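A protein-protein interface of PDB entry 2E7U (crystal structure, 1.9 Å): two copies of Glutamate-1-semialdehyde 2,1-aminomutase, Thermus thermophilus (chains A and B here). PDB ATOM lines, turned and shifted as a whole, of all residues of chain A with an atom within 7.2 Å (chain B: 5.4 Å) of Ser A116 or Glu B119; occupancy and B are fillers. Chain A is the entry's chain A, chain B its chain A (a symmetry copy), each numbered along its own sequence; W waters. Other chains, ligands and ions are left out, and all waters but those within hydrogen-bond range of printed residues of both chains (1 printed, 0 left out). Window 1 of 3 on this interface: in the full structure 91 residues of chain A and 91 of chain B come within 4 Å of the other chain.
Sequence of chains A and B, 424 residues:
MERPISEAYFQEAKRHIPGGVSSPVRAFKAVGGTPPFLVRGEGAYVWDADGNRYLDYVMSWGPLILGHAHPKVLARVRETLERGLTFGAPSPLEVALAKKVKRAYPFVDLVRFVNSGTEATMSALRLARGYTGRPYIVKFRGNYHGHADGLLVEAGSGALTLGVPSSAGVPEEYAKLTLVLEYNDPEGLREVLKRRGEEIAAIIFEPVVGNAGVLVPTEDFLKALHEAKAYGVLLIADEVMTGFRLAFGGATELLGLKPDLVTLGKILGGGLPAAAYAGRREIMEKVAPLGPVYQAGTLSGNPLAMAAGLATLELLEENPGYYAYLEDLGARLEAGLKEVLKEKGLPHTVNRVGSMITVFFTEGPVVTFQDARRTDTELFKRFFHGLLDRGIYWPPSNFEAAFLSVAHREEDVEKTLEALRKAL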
ATOM      1  N   PHE A 113     -14.868  13.325   3.885  1.00  0.00           N
ATOM      2  CA  PHE A 113     -14.967  12.360   2.792  1.00  0.00           C
ATOM      3  C   PHE A 113     -13.679  11.570   2.594  1.00  0.00           C
ATOM      4  O   PHE A 113     -12.585  12.119   2.714  1.00  0.00           O
ATOM      5  CB  PHE A 113     -15.314  13.072   1.476  1.00  0.00           C
ATOM      6  CG  PHE A 113     -16.689  13.663   1.455  1.00  0.00           C
ATOM      7  CD1 PHE A 113     -17.811  12.840   1.455  1.00  0.00           C
ATOM      8  CD2 PHE A 113     -16.868  15.044   1.484  1.00  0.00           C
ATOM      9  CE1 PHE A 113     -19.095  13.378   1.489  1.00  0.00           C
ATOM     10  CE2 PHE A 113     -18.147  15.597   1.519  1.00  0.00           C
ATOM     11  CZ  PHE A 113     -19.265  14.764   1.522  1.00  0.00           C
ATOM     12  N   VAL A 114     -13.833  10.282   2.294  1.00  0.00           N
ATOM     13  CA  VAL A 114     -12.721   9.375   2.027  1.00  0.00           C
ATOM     14  C   VAL A 114     -13.107   8.563   0.788  1.00  0.00           C
ATOM     15  O   VAL A 114     -14.208   8.729   0.264  1.00  0.00           O
ATOM     16  CB  VAL A 114     -12.449   8.436   3.229  1.00  0.00           C
ATOM     17  CG1 VAL A 114     -11.927   9.256   4.405  1.00  0.00           C
ATOM     18  CG2 VAL A 114     -13.726   7.704   3.626  1.00  0.00           C
ATOM     19  N   ASN A 115     -12.226   7.684   0.321  1.00  0.00           N
ATOM     20  CA  ASN A 115     -12.515   6.922  -0.893  1.00  0.00           C
ATOM     21  C   ASN A 115     -13.222   5.580  -0.762  1.00  0.00           C
ATOM     22  O   ASN A 115     -13.690   5.033  -1.762  1.00  0.00           O
ATOM     23  CB  ASN A 115     -11.231   6.704  -1.691  1.00  0.00           C
ATOM     24  CG  ASN A 115     -10.495   7.993  -1.963  1.00  0.00           C
ATOM     25  OD1 ASN A 115      -9.653   8.426  -1.164  1.00  0.00           O
ATOM     26  ND2 ASN A 115     -10.817   8.630  -3.083  1.00  0.00           N
ATOM     27  N   SER A 116     -13.305   5.034   0.445  1.00  0.00           N
ATOM     28  CA  SER A 116     -13.952   3.738   0.596  1.00  0.00           C
ATOM     29  C   SER A 116     -14.471   3.508   2.003  1.00  0.00           C
ATOM     30  O   SER A 116     -14.071   4.192   2.944  1.00  0.00           O
ATOM     31  CB  SER A 116     -12.965   2.626   0.249  1.00  0.00           C
ATOM     32  OG  SER A 116     -11.918   2.585   1.209  1.00  0.00           O
ATOM     33  N   GLY A 117     -15.359   2.532   2.138  1.00  0.00           N
ATOM     34  CA  GLY A 117     -15.908   2.215   3.443  1.00  0.00           C
ATOM     35  C   GLY A 117     -14.796   1.788   4.380  1.00  0.00           C
ATOM     36  O   GLY A 117     -14.817   2.126   5.561  1.00  0.00           O
ATOM     37  N   THR A 118     -13.827   1.043   3.850  1.00  0.00           N
ATOM     38  CA  THR A 118     -12.692   0.568   4.645  1.00  0.00           C
ATOM     39  C   THR A 118     -11.942   1.750   5.256  1.00  0.00           C
ATOM     40  O   THR A 118     -11.570   1.717   6.430  1.00  0.00           O
ATOM     41  CB  THR A 118     -11.713  -0.279   3.780  1.00  0.00           C
ATOM     42  OG1 THR A 118     -12.323  -1.541   3.466  1.00  0.00           O
ATOM     43  CG2 THR A 118     -10.401  -0.532   4.526  1.00  0.00           C
ATOM     44  N   GLU A 119     -11.720   2.796   4.463  1.00  0.00           N
ATOM     45  CA  GLU A 119     -11.021   3.974   4.965  1.00  0.00           C
ATOM     46  C   GLU A 119     -11.887   4.730   5.969  1.00  0.00           C
ATOM     47  O   GLU A 119     -11.380   5.248   6.961  1.00  0.00           O
ATOM     48  CB  GLU A 119     -10.648   4.925   3.822  1.00  0.00           C
ATOM     49  CG  GLU A 119      -9.724   4.339   2.776  1.00  0.00           C
ATOM     50  CD  GLU A 119      -9.237   5.393   1.788  1.00  0.00           C
ATOM     51  OE1 GLU A 119     -10.009   6.332   1.488  1.00  0.00           O
ATOM     52  OE2 GLU A 119      -8.089   5.275   1.308  1.00  0.00           O
ATOM     53  N   ALA A 120     -13.191   4.793   5.710  1.00  0.00           N
ATOM     54  CA  ALA A 120     -14.110   5.501   6.607  1.00  0.00           C
ATOM     55  C   ALA A 120     -14.149   4.887   8.001  1.00  0.00           C
ATOM     56  O   ALA A 120     -14.061   5.596   9.002  1.00  0.00           O
ATOM     57  CB  ALA A 120     -15.525   5.522   6.012  1.00  0.00           C
ATOM     58  N   THR A 121     -14.288   3.568   8.070  1.00  0.00           N
ATOM     59  CA  THR A 121     -14.355   2.899   9.366  1.00  0.00           C
ATOM     60  C   THR A 121     -12.999   2.908  10.069  1.00  0.00           C
ATOM     61  O   THR A 121     -12.920   3.082  11.279  1.00  0.00           O
ATOM     62  CB  THR A 121     -14.879   1.452   9.210  1.00  0.00           C
ATOM     63  OG1 THR A 121     -14.030   0.721   8.321  1.00  0.00           O
ATOM     64  CG2 THR A 121     -16.293   1.464   8.646  1.00  0.00           C
ATOM     65  N   MET A 122     -11.931   2.734   9.306  1.00  0.00           N
ATOM     66  CA  MET A 122     -10.586   2.756   9.869  1.00  0.00           C
ATOM     67  C   MET A 122     -10.330   4.121  10.524  1.00  0.00           C
ATOM     68  O   MET A 122      -9.783   4.207  11.628  1.00  0.00           O
ATOM     69  CB  MET A 122      -9.570   2.487   8.752  1.00  0.00           C
ATOM     70  CG  MET A 122      -8.118   2.433   9.184  1.00  0.00           C
ATOM     71  SD  MET A 122      -7.074   1.774   7.849  1.00  0.00           S
ATOM     72  CE  MET A 122      -6.843   3.215   6.823  1.00  0.00           C
ATOM     73  N   HIS A 145     -16.883  -4.203   8.266  1.00  0.00           N
ATOM     74  CA  HIS A 145     -16.705  -2.762   8.138  1.00  0.00           C
ATOM     75  C   HIS A 145     -15.539  -2.389   7.234  1.00  0.00           C
ATOM     76  O   HIS A 145     -15.208  -1.212   7.096  1.00  0.00           O
ATOM     77  CB  HIS A 145     -16.475  -2.168   9.527  1.00  0.00           C
ATOM     78  CG  HIS A 145     -17.489  -2.605  10.537  1.00  0.00           C
ATOM     79  ND1 HIS A 145     -18.811  -2.221  10.476  1.00  0.00           N
ATOM     80  CD2 HIS A 145     -17.387  -3.439  11.600  1.00  0.00           C
ATOM     81  CE1 HIS A 145     -19.480  -2.802  11.456  1.00  0.00           C
ATOM     82  NE2 HIS A 145     -18.639  -3.547  12.153  1.00  0.00           N
ATOM     83  N   HIS A 147     -11.554  -4.002   5.417  1.00  0.00           N
ATOM     84  CA  HIS A 147     -10.445  -4.878   5.740  1.00  0.00           C
ATOM     85  C   HIS A 147      -9.263  -4.291   6.501  1.00  0.00           C
ATOM     86  O   HIS A 147      -8.134  -4.715   6.295  1.00  0.00           O
ATOM     87  CB  HIS A 147      -9.954  -5.590   4.472  1.00  0.00           C
ATOM     88  CG  HIS A 147      -9.403  -4.673   3.425  1.00  0.00           C
ATOM     89  ND1 HIS A 147      -8.049  -4.512   3.215  1.00  0.00           N
ATOM     90  CD2 HIS A 147     -10.021  -3.885   2.512  1.00  0.00           C
ATOM     91  CE1 HIS A 147      -7.858  -3.666   2.218  1.00  0.00           C
ATOM     92  NE2 HIS A 147      -9.038  -3.271   1.774  1.00  0.00           N
ATOM     93  N   VAL A 240     -22.720   2.442   5.999  1.00  0.00           N
ATOM     94  CA  VAL A 240     -22.251   2.409   4.621  1.00  0.00           C
ATOM     95  C   VAL A 240     -23.308   1.767   3.728  1.00  0.00           C
ATOM     96  O   VAL A 240     -23.530   2.202   2.601  1.00  0.00           O
ATOM     97  CB  VAL A 240     -20.920   1.630   4.492  1.00  0.00           C
ATOM     98  CG1 VAL A 240     -20.630   1.316   3.032  1.00  0.00           C
ATOM     99  CG2 VAL A 240     -19.783   2.457   5.079  1.00  0.00           C
ATOM    100  N   LEU A 264     -20.465   6.480   6.265  1.00  0.00           N
ATOM    101  CA  LEU A 264     -21.361   6.429   5.117  1.00  0.00           C
ATOM    102  C   LEU A 264     -20.610   6.044   3.850  1.00  0.00           C
ATOM    103  O   LEU A 264     -19.384   6.123   3.794  1.00  0.00           O
ATOM    104  CB  LEU A 264     -22.033   7.796   4.938  1.00  0.00           C
ATOM    105  CG  LEU A 264     -22.853   8.288   6.142  1.00  0.00           C
ATOM    106  CD1 LEU A 264     -23.123   9.789   6.021  1.00  0.00           C
ATOM    107  CD2 LEU A 264     -24.163   7.509   6.226  1.00  0.00           C
ATOM    108  N   GLY A 265     -21.360   5.623   2.837  1.00  0.00           N
ATOM    109  CA  GLY A 265     -20.757   5.223   1.582  1.00  0.00           C
ATOM    110  C   GLY A 265     -21.813   4.755   0.602  1.00  0.00           C
ATOM    111  O   GLY A 265     -22.979   5.122   0.724  1.00  0.00           O
ATOM    112  N   PRO A 273     -17.022   5.533  -6.356  1.00  0.00           N
ATOM    113  CA  PRO A 273     -16.329   5.420  -5.069  1.00  0.00           C
ATOM    114  C   PRO A 273     -16.350   6.686  -4.223  1.00  0.00           C
ATOM    115  O   PRO A 273     -15.839   7.728  -4.628  1.00  0.00           O
ATOM    116  CB  PRO A 273     -14.912   5.020  -5.476  1.00  0.00           C
ATOM    117  CG  PRO A 273     -15.143   4.232  -6.740  1.00  0.00           C
ATOM    118  CD  PRO A 273     -16.139   5.110  -7.457  1.00  0.00           C
ATOM    119  N   ALA A 274     -16.954   6.581  -3.045  1.00  0.00           N
ATOM    120  CA  ALA A 274     -17.033   7.697  -2.109  1.00  0.00           C
ATOM    121  C   ALA A 274     -17.538   7.172  -0.777  1.00  0.00           C
ATOM    122  O   ALA A 274     -18.403   6.297  -0.738  1.00  0.00           O
ATOM    123  CB  ALA A 274     -17.974   8.771  -2.632  1.00  0.00           C
ATOM    124  N   ALA A 275     -16.989   7.699   0.312  1.00  0.00           N
ATOM    125  CA  ALA A 275     -17.400   7.291   1.648  1.00  0.00           C
ATOM    126  C   ALA A 275     -17.127   8.448   2.595  1.00  0.00           C
ATOM    127  O   ALA A 275     -16.558   9.468   2.196  1.00  0.00           O
ATOM    128  CB  ALA A 275     -16.625   6.050   2.082  1.00  0.00           C
ATOM    129  N   ALA A 276     -17.525   8.304   3.850  1.00  0.00           N
ATOM    130  CA  ALA A 276     -17.290   9.378   4.796  1.00  0.00           C
ATOM    131  C   ALA A 276     -17.517   8.949   6.232  1.00  0.00           C
ATOM    132  O   ALA A 276     -18.102   7.898   6.497  1.00  0.00           O
ATOM    133  CB  ALA A 276     -18.211  10.561   4.467  1.00  0.00           C
ATOM    134  N   SER A 300      -9.476  12.093  -2.456  1.00  0.00           N
ATOM    135  CA  SER A 300     -10.767  12.080  -1.776  1.00  0.00           C
ATOM    136  C   SER A 300     -11.617  13.239  -2.283  1.00  0.00           C
ATOM    137  O   SER A 300     -11.088  14.253  -2.731  1.00  0.00           O
ATOM    138  CB  SER A 300     -10.578  12.218  -0.263  1.00  0.00           C
ATOM    139  OG  SER A 300      -9.891  11.098   0.267  1.00  0.00           O
ATOM    140  N   VAL B 114      -7.561  -1.858  -6.172  1.00  0.00           N
ATOM    141  CA  VAL B 114      -8.189  -1.366  -4.948  1.00  0.00           C
ATOM    142  C   VAL B 114      -8.560   0.096  -5.205  1.00  0.00           C
ATOM    143  O   VAL B 114      -8.268   0.626  -6.276  1.00  0.00           O
ATOM    144  CB  VAL B 114      -7.235  -1.480  -3.733  1.00  0.00           C
ATOM    145  CG1 VAL B 114      -6.998  -2.953  -3.411  1.00  0.00           C
ATOM    146  CG2 VAL B 114      -5.910  -0.790  -4.036  1.00  0.00           C
ATOM    147  N   ASN B 115      -9.187   0.757  -4.236  1.00  0.00           N
ATOM    148  CA  ASN B 115      -9.619   2.138  -4.445  1.00  0.00           C
ATOM    149  C   ASN B 115      -8.662   3.265  -4.082  1.00  0.00           C
ATOM    150  O   ASN B 115      -8.894   4.414  -4.463  1.00  0.00           O
ATOM    151  CB  ASN B 115     -10.939   2.387  -3.718  1.00  0.00           C
ATOM    152  CG  ASN B 115     -11.998   1.376  -4.083  1.00  0.00           C
ATOM    153  OD1 ASN B 115     -12.113   0.319  -3.447  1.00  0.00           O
ATOM    154  ND2 ASN B 115     -12.770   1.679  -5.121  1.00  0.00           N
ATOM    155  N   SER B 116      -7.596   2.967  -3.349  1.00  0.00           N
ATOM    156  CA  SER B 116      -6.677   4.030  -2.965  1.00  0.00           C
ATOM    157  C   SER B 116      -5.286   3.510  -2.652  1.00  0.00           C
ATOM    158  O   SER B 116      -5.094   2.317  -2.424  1.00  0.00           O
ATOM    159  CB  SER B 116      -7.217   4.757  -1.736  1.00  0.00           C
ATOM    160  OG  SER B 116      -7.207   3.891  -0.610  1.00  0.00           O
ATOM    161  N   GLY B 117      -4.321   4.421  -2.635  1.00  0.00           N
ATOM    162  CA  GLY B 117      -2.956   4.036  -2.329  1.00  0.00           C
ATOM    163  C   GLY B 117      -2.886   3.447  -0.935  1.00  0.00           C
ATOM    164  O   GLY B 117      -2.148   2.493  -0.701  1.00  0.00           O
ATOM    165  N   THR B 118      -3.655   4.020  -0.010  1.00  0.00           N
ATOM    166  CA  THR B 118      -3.685   3.546   1.376  1.00  0.00           C
ATOM    167  C   THR B 118      -4.100   2.077   1.424  1.00  0.00           C
ATOM    168  O   THR B 118      -3.508   1.280   2.153  1.00  0.00           O
ATOM    169  CB  THR B 118      -4.663   4.392   2.241  1.00  0.00           C
ATOM    170  OG1 THR B 118      -4.105   5.699   2.453  1.00  0.00           O
ATOM    171  CG2 THR B 118      -4.909   3.730   3.598  1.00  0.00           C
ATOM    172  N   GLU B 119      -5.119   1.715   0.646  1.00  0.00           N
ATOM    173  CA  GLU B 119      -5.577   0.329   0.619  1.00  0.00           C
ATOM    174  C   GLU B 119      -4.546  -0.568  -0.060  1.00  0.00           C
ATOM    175  O   GLU B 119      -4.336  -1.702   0.363  1.00  0.00           O
ATOM    176  CB  GLU B 119      -6.909   0.203  -0.130  1.00  0.00           C
ATOM    177  CG  GLU B 119      -8.059   0.983   0.471  1.00  0.00           C
ATOM    178  CD  GLU B 119      -9.387   0.652  -0.201  1.00  0.00           C
ATOM    179  OE1 GLU B 119      -9.386   0.375  -1.422  1.00  0.00           O
ATOM    180  OE2 GLU B 119     -10.428   0.677   0.491  1.00  0.00           O
ATOM    181  N   ALA B 120      -3.906  -0.060  -1.110  1.00  0.00           N
ATOM    182  CA  ALA B 120      -2.901  -0.843  -1.837  1.00  0.00           C
ATOM    183  C   ALA B 120      -1.712  -1.216  -0.963  1.00  0.00           C
ATOM    184  O   ALA B 120      -1.283  -2.370  -0.945  1.00  0.00           O
ATOM    185  CB  ALA B 120      -2.412  -0.068  -3.070  1.00  0.00           C
ATOM    186  N   THR B 121      -1.171  -0.243  -0.239  1.00  0.00           N
ATOM    187  CA  THR B 121      -0.015  -0.508   0.612  1.00  0.00           C
ATOM    188  C   THR B 121      -0.399  -1.353   1.826  1.00  0.00           C
ATOM    189  O   THR B 121       0.345  -2.234   2.239  1.00  0.00           O
ATOM    190  CB  THR B 121       0.655   0.813   1.057  1.00  0.00           C
ATOM    191  OG1 THR B 121      -0.292   1.627   1.752  1.00  0.00           O
ATOM    192  CG2 THR B 121       1.168   1.575  -0.157  1.00  0.00           C
ATOM    193  N   MET B 122      -1.570  -1.091   2.388  1.00  0.00           N
ATOM    194  CA  MET B 122      -2.049  -1.857   3.532  1.00  0.00           C
ATOM    195  C   MET B 122      -2.171  -3.337   3.140  1.00  0.00           C
ATOM    196  O   MET B 122      -1.777  -4.232   3.894  1.00  0.00           O
ATOM    197  CB  MET B 122      -3.404  -1.296   3.979  1.00  0.00           C
ATOM    198  CG  MET B 122      -4.022  -1.960   5.194  1.00  0.00           C
ATOM    199  SD  MET B 122      -5.429  -0.988   5.812  1.00  0.00           S
ATOM    200  CE  MET B 122      -6.737  -1.504   4.713  1.00  0.00           C
ATOM    201  N   SER B 123      -2.705  -3.589   1.947  1.00  0.00           N
ATOM    202  CA  SER B 123      -2.875  -4.950   1.452  1.00  0.00           C
ATOM    203  C   SER B 123      -1.536  -5.612   1.143  1.00  0.00           C
ATOM    204  O   SER B 123      -1.335  -6.788   1.450  1.00  0.00           O
ATOM    205  CB  SER B 123      -3.727  -4.966   0.176  1.00  0.00           C
ATOM    206  OG  SER B 123      -4.997  -4.385   0.392  1.00  0.00           O
ATOM    207  N   ALA B 124      -0.632  -4.860   0.522  1.00  0.00           N
ATOM    208  CA  ALA B 124       0.673  -5.396   0.154  1.00  0.00           C
ATOM    209  C   ALA B 124       1.489  -5.805   1.376  1.00  0.00           C
ATOM    210  O   ALA B 124       2.167  -6.830   1.355  1.00  0.00           O
ATOM    211  CB  ALA B 124       1.443  -4.377  -0.672  1.00  0.00           C
ATOM    212  N   TYR B 277      -1.947  -3.426  -6.225  1.00  0.00           N
ATOM    213  CA  TYR B 277      -0.738  -4.051  -5.709  1.00  0.00           C
ATOM    214  C   TYR B 277      -0.562  -5.254  -6.621  1.00  0.00           C
ATOM    215  O   TYR B 277      -1.547  -5.882  -7.022  1.00  0.00           O
ATOM    216  CB  TYR B 277      -0.851  -4.427  -4.218  1.00  0.00           C
ATOM    217  CG  TYR B 277      -1.970  -5.356  -3.799  1.00  0.00           C
ATOM    218  CD1 TYR B 277      -3.250  -4.865  -3.550  1.00  0.00           C
ATOM    219  CD2 TYR B 277      -1.726  -6.706  -3.558  1.00  0.00           C
ATOM    220  CE1 TYR B 277      -4.260  -5.692  -3.063  1.00  0.00           C
ATOM    221  CE2 TYR B 277      -2.731  -7.549  -3.066  1.00  0.00           C
ATOM    222  CZ  TYR B 277      -3.992  -7.030  -2.820  1.00  0.00           C
ATOM    223  OH  TYR B 277      -4.979  -7.838  -2.305  1.00  0.00           O
ATOM    224  N   SER B 300     -14.252  -1.663  -6.026  1.00  0.00           N
ATOM    225  CA  SER B 300     -12.939  -1.668  -6.663  1.00  0.00           C
ATOM    226  C   SER B 300     -13.100  -1.959  -8.150  1.00  0.00           C
ATOM    227  O   SER B 300     -14.065  -2.598  -8.562  1.00  0.00           O
ATOM    228  CB  SER B 300     -12.043  -2.740  -6.036  1.00  0.00           C
ATOM    229  OG  SER B 300     -11.773  -2.442  -4.677  1.00  0.00           O
HETATM  230  O   HOH W   1      -9.868  -2.137  -0.673  1.00  0.00           O
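Glu B119 touches two residues of chain A. Of the printed residues of chain A, Asn B115 touches Pro A273. Of the printed residues of chain B, Thr A118 touches Glu B119 and Met B122. Printed residues of chain A within 4 Å of Ser B116: Glu A119. Printed residues of chain B within 4 Å of His A147: Met B122 and Ser B123. Ala A275 touches none of the printed residues of chain B. The nearest printed residue of chain B that does not touch Thr A118 is Thr B118 (7.0 Å).
Ser A116 touches Glu B119, and with the chains exchanged Glu A119 touches Ser B116. Thr A118 touches Glu B119, and with the chains exchanged Glu A119 touches Thr B118. Thr A118 touches Met B122, and with the chains exchanged Met A122 touches Thr B118. Met A122 touches its own counterpart, Met B122. Of the 10 pairs that touch across the chains among the printed residues, 7 have their exchanged pair printed and touching as well.
Water W1 bridges the side-chain carboxylate of Glu B119 (2.7 Å) and a ring nitrogen (NE2) of His A147 (2.8 Å).
The backbone NH (N) of Asn A115 lies within hydrogen-bond range of the side-chain carboxylate (OE1) of Glu A119, 2.8 Å away. O of Thr A118 is in hydrogen-bond range of OG1 of Thr A121 (3.3 Å). The side-chain hydroxyl (OG1) of Thr A118 lies within hydrogen-bond range of the backbone NH (N) of His A147. The side-chain amide oxygen (OD1) of Asn B115 lies within hydrogen-bond range of the side-chain hydroxyl (OG) of Ser B300 (3.0 Å). The side-chain hydroxyl (OG) of Ser B116 sits close to the backbone NH (N) of Glu B119, at 3.3 Å. O of Thr B118 sits at hydrogen-bond distance from OG1 of Thr B121.
Of the 13 printed residues of chain B, 6 touch a printed residue of chain A. Hydrophobic or aromatic side chains of chain B within 4 Å of the printed part of chain A: Met B122. Along chain A the printed residues that touch a printed residue of chain B span positions 116 to 273. Among the printed residues, no Asp or Glu carboxylate lies within 4 Å of a Lys or Arg side-chain nitrogen of the other chain.
OE2 of Glu B119 is in hydrogen-bond range of OG of Ser A116, 2.5 Å away. The side-chain carboxylate (OE2) of Glu A119 is in hydrogen-bond range of the side-chain hydroxyl (OG) of Ser B116, 2.5 Å away.
Glu B119 touches Thr A118. Met B122 touches Thr A118 (CE to CG2, 3.8 Å). OE2 of Glu A119 touches CB of Thr B118, at 3.7 Å. CE of Met A122 touches CG2 of Thr B118, at 3.8 Å. Met A122 touches Met B122 (SD to SD, 3.8 Å). CE of Met B122 touches CE1 of His A147, 3.5 Å away. CE1 of His A147 touches OG of Ser B123 (3.5 Å). CG of Pro A273 touches ND2 of Asn B115, at 3.8 Å.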
